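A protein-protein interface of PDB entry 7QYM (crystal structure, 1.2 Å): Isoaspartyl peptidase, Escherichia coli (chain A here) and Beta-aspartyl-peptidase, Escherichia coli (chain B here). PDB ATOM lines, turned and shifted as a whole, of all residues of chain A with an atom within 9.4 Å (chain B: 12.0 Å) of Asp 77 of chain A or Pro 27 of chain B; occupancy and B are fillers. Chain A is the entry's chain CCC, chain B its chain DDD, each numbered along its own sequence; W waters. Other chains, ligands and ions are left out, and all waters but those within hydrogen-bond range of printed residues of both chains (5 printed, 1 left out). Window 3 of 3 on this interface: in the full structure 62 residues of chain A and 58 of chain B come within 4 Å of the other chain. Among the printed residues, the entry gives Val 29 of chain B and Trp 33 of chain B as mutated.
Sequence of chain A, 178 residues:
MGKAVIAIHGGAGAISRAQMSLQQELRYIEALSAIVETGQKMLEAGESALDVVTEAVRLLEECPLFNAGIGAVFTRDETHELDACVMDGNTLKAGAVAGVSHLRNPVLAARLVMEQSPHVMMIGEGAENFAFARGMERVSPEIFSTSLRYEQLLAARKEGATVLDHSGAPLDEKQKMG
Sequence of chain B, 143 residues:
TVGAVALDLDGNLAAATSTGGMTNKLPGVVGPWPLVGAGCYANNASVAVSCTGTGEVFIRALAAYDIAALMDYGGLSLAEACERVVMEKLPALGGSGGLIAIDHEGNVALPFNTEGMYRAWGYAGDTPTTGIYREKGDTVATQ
The backbone carbonyl oxygen (O) of Val 73 of chain A sits at hydrogen-bond distance from a ring nitrogen (ND1) of His 80 of chain A (2.8 Å).
The side-chain hydroxyl (OG1) of Thr 75 of chain A sits close to the backbone NH (N) of Asp 77 of chain A (3.1 Å).
The side-chain hydroxyl of Thr 79 of chain A sits at hydrogen-bond distance from the side-chain hydroxyl of Thr 75 of chain A (2.6 Å).
The side-chain amino group (NZ) of Lys 25 of chain B lies within hydrogen-bond range of the backbone carbonyl oxygen (O) of Val 29 of chain B, at 3.1 Å.
Of the 13 printed residues of chain B, 9 touch a printed residue of chain A.
Hydrophobic or aromatic side chains of chain B that line the printed part of chain A: Leu 26 and Pro 27.
Among the printed residues, Asp or Glu carboxylates within 4 Å of a Lys or Arg side-chain nitrogen of the other chain: Glu 81 of chain A with Lys 25 of chain B (3.6 Å).
Water W4 lies within hydrogen-bond range of OD2 of Asp 83 of chain A (2.6 Å) and N of Gly 31 of chain B (2.8 Å).
Water W3 lies within hydrogen-bond range of OD1 of Asp 83 of chain A (2.7 Å), O of Val 29 of chain B (2.9 Å) and NZ of Lys 25 of chain B (3.3 Å).
Water W2 lies within hydrogen-bond range of O of Gly 20 of chain B, O of Val 73 of chain A and N of Glu 81 of chain A.
Water W1 lies within hydrogen-bond range of OE2 of Glu 81 of chain A (2.8 Å) and N of Gly 28 of chain B (3.3 Å).
Water W5 lies within hydrogen-bond range of the side-chain hydroxyl of Thr 23 of chain B (2.8 Å) and the backbone NH of Phe 74 of chain A (2.9 Å).
O of Phe 74 of chain A is in hydrogen-bond range of N of Asn 24 of chain B.
The guanidinium group of Arg 76 of chain A sits at hydrogen-bond distance from the backbone carbonyl oxygen of Asn 24 of chain B, at 2.9 Å.
O of Lys 25 of chain B sits at hydrogen-bond distance from N of Arg 76 of chain A (2.9 Å).
The side-chain amino group of Lys 25 of chain B lies within salt-bridge range of the side-chain carboxylate of Glu 81 of chain A (3.6 Å).
The backbone NH (N) of Gly 28 of chain B is in hydrogen-bond range of the side-chain carboxylate (OE1) of Glu 81 of chain A (2.9 Å).
The backbone carbonyl oxygen (O) of Glu 81 of chain A lies close to the backbone carbonyl oxygen (O) of Gly 20 of chain B, 3.3 Å away.
O of Gly 20 of chain B touches CG2 of Val 73 of chain A, at 3.4 Å.
Val 73 of chain A touches Gly 21 of chain B.
Val 73 of chain A touches Met 22 of chain B (CG2 to C, 3.5 Å).
Thr 23 of chain B touches Val 73 of chain A.
O of Phe 74 of chain A touches CA of Thr 23 of chain B, 3.4 Å away.
Thr 75 of chain A touches Lys 25 of chain B.
Pro 27 of chain B touches Asp 77 of chain A (CG to OD2, 3.4 Å).
Glu 81 of chain A touches Pro 27 of chain B (OE2 to CB, 3.3 Å).
CA of Leu 153 of chain A touches CG2 of Thr 23 of chain B (3.8 Å).
Asn 24 of chain B touches Leu 153 of chain A (OD1 to CD1, 3.7 Å).
Printed residues of chain B within 4 Å of Asp 77 of chain A: Pro 27.
Pro 27 of chain B touches just these residues of chain A: Asp 77 and Glu 81.
No residue of chain B comes within 4 Å of Glu 78 of chain A.
No residue of chain B comes within 4 Å of Thr 79 of chain A.
Of the printed residues of chain A, Leu 26 of chain B touches Arg 76 (3.7 Å).
Printed residues of chain A within 4 Å of Gly 21 of chain B: Val 73.
Of the printed residues of chain A, Thr 23 of chain B touches Val 73, Phe 74 and Leu 153.
Tyr 150 of chain A touches none of the printed residues of chain B.
The nearest printed residue of chain B that does not touch Arg 76 of chain A is Pro 27 of chain B (4.4 Å).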
ATOM      1  N   VAL A  73      -2.941  -7.986 -25.640  1.00  0.00           N
ATOM      2  CA  VAL A  73      -2.328  -8.939 -24.705  1.00  0.00           C
ATOM      3  C   VAL A  73      -2.393  -8.400 -23.287  1.00  0.00           C
ATOM      4  O   VAL A  73      -2.643  -7.215 -23.035  1.00  0.00           O
ATOM      5  CB  VAL A  73      -0.893  -9.256 -25.105  1.00  0.00           C
ATOM      6  CG1 VAL A  73      -0.822  -9.996 -26.438  1.00  0.00           C
ATOM      7  CG2 VAL A  73      -0.006  -8.008 -25.119  1.00  0.00           C
ATOM      8  N   PHE A  74      -2.212  -9.328 -22.363  1.00  0.00           N
ATOM      9  CA  PHE A  74      -2.149  -9.028 -20.932  1.00  0.00           C
ATOM     10  C   PHE A  74      -0.712  -8.822 -20.491  1.00  0.00           C
ATOM     11  O   PHE A  74       0.158  -9.591 -20.915  1.00  0.00           O
ATOM     12  CB  PHE A  74      -2.765 -10.173 -20.136  1.00  0.00           C
ATOM     13  CG  PHE A  74      -4.255 -10.322 -20.275  1.00  0.00           C
ATOM     14  CD1 PHE A  74      -4.848 -10.975 -21.352  1.00  0.00           C
ATOM     15  CD2 PHE A  74      -5.082  -9.749 -19.329  1.00  0.00           C
ATOM     16  CE1 PHE A  74      -6.227 -11.125 -21.414  1.00  0.00           C
ATOM     17  CE2 PHE A  74      -6.457  -9.897 -19.384  1.00  0.00           C
ATOM     18  CZ  PHE A  74      -7.032 -10.588 -20.426  1.00  0.00           C
ATOM     19  N   THR A  75      -0.479  -7.850 -19.624  1.00  0.00           N
ATOM     20  CA  THR A  75       0.808  -7.658 -18.945  1.00  0.00           C
ATOM     21  C   THR A  75       0.988  -8.726 -17.857  1.00  0.00           C
ATOM     22  O   THR A  75       0.045  -9.523 -17.580  1.00  0.00           O
ATOM     23  CB  THR A  75       0.904  -6.287 -18.265  1.00  0.00           C
ATOM     24  OG1 THR A  75       0.076  -6.349 -17.099  1.00  0.00           O
ATOM     25  CG2 THR A  75       0.516  -5.148 -19.191  1.00  0.00           C
ATOM     26  N   ARG A  76       2.190  -8.744 -17.270  1.00  0.00           N
ATOM     27  CA  ARG A  76       2.521  -9.594 -16.110  1.00  0.00           C
ATOM     28  C   ARG A  76       1.475  -9.459 -15.002  1.00  0.00           C
ATOM     29  O   ARG A  76       1.262 -10.445 -14.223  1.00  0.00           O
ATOM     30  CB  ARG A  76       3.895  -9.199 -15.555  1.00  0.00           C
ATOM     31  CG  ARG A  76       4.520 -10.309 -14.738  1.00  0.00           C
ATOM     32  CD  ARG A  76       6.013 -10.308 -14.841  1.00  0.00           C
ATOM     33  NE  ARG A  76       6.518 -10.160 -16.193  1.00  0.00           N
ATOM     34  CZ  ARG A  76       7.741  -9.742 -16.455  1.00  0.00           C
ATOM     35  NH1 ARG A  76       8.549  -9.471 -15.449  1.00  0.00           N
ATOM     36  NH2 ARG A  76       8.153  -9.605 -17.702  1.00  0.00           N
ATOM     37  N   ASP A  77       0.907  -8.277 -14.845  1.00  0.00           N
ATOM     38  CA  ASP A  77      -0.065  -7.974 -13.765  1.00  0.00           C
ATOM     39  C   ASP A  77      -1.513  -8.218 -14.222  1.00  0.00           C
ATOM     40  O   ASP A  77      -2.427  -7.774 -13.490  1.00  0.00           O
ATOM     41  CB  ASP A  77       0.108  -6.544 -13.260  1.00  0.00           C
ATOM     42  CG  ASP A  77       1.387  -6.325 -12.478  1.00  0.00           C
ATOM     43  OD1 ASP A  77       2.040  -7.335 -12.150  1.00  0.00           O
ATOM     44  OD2 ASP A  77       1.667  -5.157 -12.124  1.00  0.00           O
ATOM     45  N   GLU A  78      -1.738  -8.869 -15.366  1.00  0.00           N
ATOM     46  CA  GLU A  78      -3.100  -9.157 -15.888  1.00  0.00           C
ATOM     47  C   GLU A  78      -3.813  -7.841 -16.179  1.00  0.00           C
ATOM     48  O   GLU A  78      -5.032  -7.778 -16.008  1.00  0.00           O
ATOM     49  CB  GLU A  78      -3.941 -10.035 -14.967  1.00  0.00           C
ATOM     50  CG  GLU A  78      -3.290 -11.336 -14.648  1.00  0.00           C
ATOM     51  CD  GLU A  78      -4.155 -12.341 -13.912  1.00  0.00           C
ATOM     52  OE1 GLU A  78      -5.396 -12.241 -13.940  1.00  0.00           O
ATOM     53  OE2 GLU A  78      -3.558 -13.170 -13.256  1.00  0.00           O
ATOM     54  N   THR A  79      -3.051  -6.838 -16.603  1.00  0.00           N
ATOM     55  CA  THR A  79      -3.563  -5.516 -17.017  1.00  0.00           C
ATOM     56  C   THR A  79      -3.408  -5.421 -18.541  1.00  0.00           C
ATOM     57  O   THR A  79      -2.750  -6.267 -19.187  1.00  0.00           O
ATOM     58  CB  THR A  79      -2.879  -4.366 -16.236  1.00  0.00           C
ATOM     59  OG1 THR A  79      -1.481  -4.329 -16.590  1.00  0.00           O
ATOM     60  CG2 THR A  79      -3.002  -4.494 -14.732  1.00  0.00           C
ATOM     61  N   HIS A  80      -3.917  -4.354 -19.098  1.00  0.00           N
ATOM     62  CA  HIS A  80      -3.628  -3.971 -20.482  1.00  0.00           C
ATOM     63  C   HIS A  80      -2.992  -2.582 -20.447  1.00  0.00           C
ATOM     64  O   HIS A  80      -3.516  -1.700 -19.755  1.00  0.00           O
ATOM     65  CB  HIS A  80      -4.894  -4.000 -21.319  1.00  0.00           C
ATOM     66  CG  HIS A  80      -5.618  -5.290 -21.329  1.00  0.00           C
ATOM     67  ND1 HIS A  80      -5.141  -6.427 -21.962  1.00  0.00           N
ATOM     68  CD2 HIS A  80      -6.801  -5.616 -20.775  1.00  0.00           C
ATOM     69  CE1 HIS A  80      -6.005  -7.411 -21.745  1.00  0.00           C
ATOM     70  NE2 HIS A  80      -7.046  -6.924 -21.057  1.00  0.00           N
ATOM     71  N   GLU A  81      -1.947  -2.415 -21.227  1.00  0.00           N
ATOM     72  CA  GLU A  81      -1.262  -1.121 -21.424  1.00  0.00           C
ATOM     73  C   GLU A  81      -1.128  -0.957 -22.923  1.00  0.00           C
ATOM     74  O   GLU A  81      -0.460  -1.782 -23.555  1.00  0.00           O
ATOM     75  CB  GLU A  81       0.110  -1.085 -20.743  1.00  0.00           C
ATOM     76  CG  GLU A  81       0.045  -1.069 -19.235  1.00  0.00           C
ATOM     77  CD  GLU A  81       1.387  -0.956 -18.540  1.00  0.00           C
ATOM     78  OE1 GLU A  81       2.446  -0.955 -19.203  1.00  0.00           O
ATOM     79  OE2 GLU A  81       1.386  -0.971 -17.313  1.00  0.00           O
ATOM     80  N   ASP A  83      -0.571   1.395 -26.594  1.00  0.00           N
ATOM     81  CA  ASP A  83       0.227   2.496 -27.177  1.00  0.00           C
ATOM     82  C   ASP A  83      -0.159   2.659 -28.646  1.00  0.00           C
ATOM     83  O   ASP A  83      -0.528   1.668 -29.296  1.00  0.00           O
ATOM     84  CB  ASP A  83       1.731   2.189 -27.098  1.00  0.00           C
ATOM     85  CG  ASP A  83       2.204   1.433 -25.867  1.00  0.00           C
ATOM     86  OD1 ASP A  83       2.094   1.983 -24.803  1.00  0.00           O
ATOM     87  OD2 ASP A  83       2.684   0.307 -26.019  1.00  0.00           O
ATOM     88  N   GLY A  99       1.070   3.737 -22.736  1.00  0.00           N
ATOM     89  CA  GLY A  99       0.705   3.339 -21.376  1.00  0.00           C
ATOM     90  C   GLY A  99      -0.707   3.738 -21.022  1.00  0.00           C
ATOM     91  O   GLY A  99      -0.963   4.013 -19.848  1.00  0.00           O
ATOM     92  N   SER A 101      -4.834   2.831 -20.642  1.00  0.00           N
ATOM     93  CA  SER A 101      -5.681   1.665 -20.285  1.00  0.00           C
ATOM     94  C   SER A 101      -7.176   2.011 -20.351  1.00  0.00           C
ATOM     95  O   SER A 101      -7.973   1.074 -20.283  1.00  0.00           O
ATOM     96  CB  SER A 101      -5.312   1.165 -18.894  1.00  0.00           C
ATOM     97  OG  SER A 101      -3.933   0.832 -18.811  1.00  0.00           O
ATOM     98  N   TYR A 150      -6.018 -14.249 -22.707  1.00  0.00           N
ATOM     99  CA  TYR A 150      -5.870 -14.674 -21.306  1.00  0.00           C
ATOM    100  C   TYR A 150      -5.282 -16.080 -21.268  1.00  0.00           C
ATOM    101  O   TYR A 150      -4.370 -16.332 -20.467  1.00  0.00           O
ATOM    102  CB  TYR A 150      -7.217 -14.568 -20.613  1.00  0.00           C
ATOM    103  CG  TYR A 150      -7.083 -14.792 -19.130  1.00  0.00           C
ATOM    104  CD1 TYR A 150      -6.415 -13.876 -18.326  1.00  0.00           C
ATOM    105  CD2 TYR A 150      -7.593 -15.927 -18.535  1.00  0.00           C
ATOM    106  CE1 TYR A 150      -6.257 -14.082 -16.966  1.00  0.00           C
ATOM    107  CE2 TYR A 150      -7.459 -16.143 -17.179  1.00  0.00           C
ATOM    108  CZ  TYR A 150      -6.804 -15.213 -16.396  1.00  0.00           C
ATOM    109  OH  TYR A 150      -6.671 -15.458 -15.068  1.00  0.00           O
ATOM    110  N   LEU A 153      -1.603 -15.850 -21.812  1.00  0.00           N
ATOM    111  CA  LEU A 153      -0.926 -15.467 -20.548  1.00  0.00           C
ATOM    112  C   LEU A 153      -0.793 -16.682 -19.614  1.00  0.00           C
ATOM    113  O   LEU A 153       0.310 -16.927 -19.117  1.00  0.00           O
ATOM    114  CB  LEU A 153      -1.700 -14.341 -19.873  1.00  0.00           C
ATOM    115  CG  LEU A 153      -1.039 -13.830 -18.591  1.00  0.00           C
ATOM    116  CD1 LEU A 153       0.236 -13.038 -18.886  1.00  0.00           C
ATOM    117  CD2 LEU A 153      -2.011 -12.965 -17.820  1.00  0.00           C
ATOM    118  N   ARG A 157       2.866 -19.036 -18.009  1.00  0.00           N
ATOM    119  CA  ARG A 157       3.187 -18.838 -16.587  1.00  0.00           C
ATOM    120  C   ARG A 157       2.802 -20.075 -15.774  1.00  0.00           C
ATOM    121  O   ARG A 157       2.191 -21.023 -16.319  1.00  0.00           O
ATOM    122  CB  ARG A 157       2.491 -17.570 -16.084  1.00  0.00           C
ATOM    123  CG  ARG A 157       1.011 -17.729 -15.794  1.00  0.00           C
ATOM    124  CD  ARG A 157       0.385 -16.412 -15.375  1.00  0.00           C
ATOM    125  NE  ARG A 157      -0.930 -16.637 -14.795  1.00  0.00           N
ATOM    126  CZ  ARG A 157      -1.744 -15.682 -14.360  1.00  0.00           C
ATOM    127  NH1 ARG A 157      -2.904 -16.019 -13.821  1.00  0.00           N
ATOM    128  NH2 ARG A 157      -1.395 -14.409 -14.475  1.00  0.00           N
ATOM    129  N   GLY B  20      -0.869  -3.574 -28.045  1.00  0.00           N
ATOM    130  CA  GLY B  20      -0.914  -3.950 -26.628  1.00  0.00           C
ATOM    131  C   GLY B  20       0.433  -4.342 -26.054  1.00  0.00           C
ATOM    132  O   GLY B  20       0.486  -4.661 -24.825  1.00  0.00           O
ATOM    133  N   GLY B  21       1.504  -4.381 -26.835  1.00  0.00           N
ATOM    134  CA  GLY B  21       2.819  -4.803 -26.323  1.00  0.00           C
ATOM    135  C   GLY B  21       2.937  -6.302 -26.360  1.00  0.00           C
ATOM    136  O   GLY B  21       2.390  -6.916 -27.233  1.00  0.00           O
ATOM    137  N   MET B  22       3.648  -6.876 -25.403  1.00  0.00           N
ATOM    138  CA  MET B  22       3.967  -8.326 -25.345  1.00  0.00           C
ATOM    139  C   MET B  22       3.207  -8.993 -24.189  1.00  0.00           C
ATOM    140  O   MET B  22       3.099  -8.383 -23.126  1.00  0.00           O
ATOM    141  CB  MET B  22       5.477  -8.516 -25.155  1.00  0.00           C
ATOM    142  CG  MET B  22       6.330  -7.571 -26.007  1.00  0.00           C
ATOM    143  SD  MET B  22       6.316  -7.914 -27.802  1.00  0.00           S
ATOM    144  CE  MET B  22       7.284  -9.426 -27.818  1.00  0.00           C
ATOM    145  N   THR B  23       2.731 -10.214 -24.399  1.00  0.00           N
ATOM    146  CA  THR B  23       2.153 -11.037 -23.319  1.00  0.00           C
ATOM    147  C   THR B  23       3.196 -11.062 -22.222  1.00  0.00           C
ATOM    148  O   THR B  23       4.407 -11.283 -22.481  1.00  0.00           O
ATOM    149  CB  THR B  23       1.731 -12.425 -23.796  1.00  0.00           C
ATOM    150  OG1 THR B  23       0.623 -12.270 -24.688  1.00  0.00           O
ATOM    151  CG2 THR B  23       1.400 -13.394 -22.681  1.00  0.00           C
ATOM    152  N   ASN B  24       2.717 -10.842 -21.015  1.00  0.00           N
ATOM    153  CA  ASN B  24       3.540 -10.950 -19.806  1.00  0.00           C
ATOM    154  C   ASN B  24       4.545  -9.804 -19.721  1.00  0.00           C
ATOM    155  O   ASN B  24       5.489  -9.878 -18.942  1.00  0.00           O
ATOM    156  CB  ASN B  24       4.217 -12.313 -19.788  1.00  0.00           C
ATOM    157  CG  ASN B  24       4.419 -12.773 -18.379  1.00  0.00           C
ATOM    158  OD1 ASN B  24       3.601 -12.504 -17.493  1.00  0.00           O
ATOM    159  ND2 ASN B  24       5.551 -13.409 -18.162  1.00  0.00           N
ATOM    160  N   LYS B  25       4.311  -8.703 -20.420  1.00  0.00           N
ATOM    161  CA  LYS B  25       5.260  -7.568 -20.352  1.00  0.00           C
ATOM    162  C   LYS B  25       5.277  -6.975 -18.936  1.00  0.00           C
ATOM    163  O   LYS B  25       4.238  -6.963 -18.196  1.00  0.00           O
ATOM    164  CB  LYS B  25       4.917  -6.453 -21.341  1.00  0.00           C
ATOM    165  CG  LYS B  25       3.582  -5.768 -21.084  1.00  0.00           C
ATOM    166  CD  LYS B  25       3.270  -4.624 -22.025  1.00  0.00           C
ATOM    167  CE  LYS B  25       4.008  -3.362 -21.654  1.00  0.00           C
ATOM    168  NZ  LYS B  25       3.427  -2.213 -22.382  1.00  0.00           N
ATOM    169  N   LEU B  26       6.417  -6.423 -18.574  1.00  0.00           N
ATOM    170  CA  LEU B  26       6.551  -5.671 -17.320  1.00  0.00           C
ATOM    171  C   LEU B  26       5.786  -4.362 -17.454  1.00  0.00           C
ATOM    172  O   LEU B  26       5.983  -3.641 -18.440  1.00  0.00           O
ATOM    173  CB  LEU B  26       8.028  -5.418 -17.038  1.00  0.00           C
ATOM    174  CG  LEU B  26       8.296  -4.779 -15.679  1.00  0.00           C
ATOM    175  CD1 LEU B  26       8.030  -5.762 -14.537  1.00  0.00           C
ATOM    176  CD2 LEU B  26       9.724  -4.248 -15.630  1.00  0.00           C
ATOM    177  N   PRO B  27       4.862  -4.012 -16.533  1.00  0.00           N
ATOM    178  CA  PRO B  27       4.158  -2.738 -16.655  1.00  0.00           C
ATOM    179  C   PRO B  27       5.157  -1.577 -16.741  1.00  0.00           C
ATOM    180  O   PRO B  27       6.130  -1.497 -16.029  1.00  0.00           O
ATOM    181  CB  PRO B  27       3.361  -2.703 -15.360  1.00  0.00           C
ATOM    182  CG  PRO B  27       3.058  -4.146 -15.101  1.00  0.00           C
ATOM    183  CD  PRO B  27       4.344  -4.852 -15.440  1.00  0.00           C
ATOM    184  N   GLY B  28       4.834  -0.654 -17.638  1.00  0.00           N
ATOM    185  CA  GLY B  28       5.623   0.579 -17.810  1.00  0.00           C
ATOM    186  C   GLY B  28       6.622   0.506 -18.933  1.00  0.00           C
ATOM    187  O   GLY B  28       7.267   1.494 -19.211  1.00  0.00           O
ATOM    188  N   VAL B  29       6.798  -0.645 -19.550  1.00  0.00           N
ATOM    189  CA  VAL B  29       7.716  -0.771 -20.702  1.00  0.00           C
ATOM    190  C   VAL B  29       7.056  -0.097 -21.910  1.00  0.00           C
ATOM    191  O   VAL B  29       5.859  -0.342 -22.184  1.00  0.00           O
ATOM    192  CB  VAL B  29       8.044  -2.242 -20.998  1.00  0.00           C
ATOM    193  CG1 VAL B  29       8.732  -2.419 -22.344  1.00  0.00           C
ATOM    194  CG2 VAL B  29       8.861  -2.825 -19.848  1.00  0.00           C
ATOM    195  N   VAL B  30       7.819   0.710 -22.629  1.00  0.00           N
ATOM    196  CA  VAL B  30       7.389   1.260 -23.930  1.00  0.00           C
ATOM    197  C   VAL B  30       8.331   0.708 -24.986  1.00  0.00           C
ATOM    198  O   VAL B  30       9.538   0.961 -24.922  1.00  0.00           O
ATOM    199  CB  VAL B  30       7.363   2.789 -23.902  1.00  0.00           C
ATOM    200  CG1 VAL B  30       6.901   3.314 -25.241  1.00  0.00           C
ATOM    201  CG2 VAL B  30       6.449   3.284 -22.780  1.00  0.00           C
ATOM    202  N   GLY B  31       7.747  -0.023 -25.911  1.00  0.00           N
ATOM    203  CA  GLY B  31       8.489  -0.516 -27.061  1.00  0.00           C
ATOM    204  C   GLY B  31       8.550   0.534 -28.152  1.00  0.00           C
ATOM    205  O   GLY B  31       8.204   1.707 -27.993  1.00  0.00           O
ATOM    206  N   TRP B  33       6.713   1.152 -30.663  1.00  0.00           N
ATOM    207  CA  TRP B  33       5.468   1.435 -31.449  1.00  0.00           C
ATOM    208  C   TRP B  33       4.945   2.861 -31.311  1.00  0.00           C
ATOM    209  O   TRP B  33       4.479   3.457 -32.287  1.00  0.00           O
ATOM    210  CB  TRP B  33       4.400   0.397 -31.097  1.00  0.00           C
ATOM    211  CG  TRP B  33       4.988  -0.952 -31.336  1.00  0.00           C
ATOM    212  CD1 TRP B  33       5.309  -1.491 -32.546  1.00  0.00           C
ATOM    213  CD2 TRP B  33       5.510  -1.846 -30.342  1.00  0.00           C
ATOM    214  NE1 TRP B  33       5.928  -2.697 -32.369  1.00  0.00           N
ATOM    215  CE2 TRP B  33       6.062  -2.944 -31.030  1.00  0.00           C
ATOM    216  CE3 TRP B  33       5.555  -1.827 -28.950  1.00  0.00           C
ATOM    217  CZ2 TRP B  33       6.620  -4.034 -30.362  1.00  0.00           C
ATOM    218  CZ3 TRP B  33       6.082  -2.912 -28.289  1.00  0.00           C
ATOM    219  CH2 TRP B  33       6.622  -3.992 -28.985  1.00  0.00           C
HETATM  220  O   HOH W   1       2.670   0.705 -15.474  1.00  0.00           O
HETATM  221  O   HOH W   2      -1.455  -4.720 -22.887  1.00  0.00           O
HETATM  222  O   HOH W   3       3.349   1.079 -22.553  1.00  0.00           O
HETATM  223  O   HOH W   4       5.054  -0.782 -26.275  1.00  0.00           O
HETATM  224  O   HOH W   5      -1.845 -12.065 -23.355  1.00  0.00           O
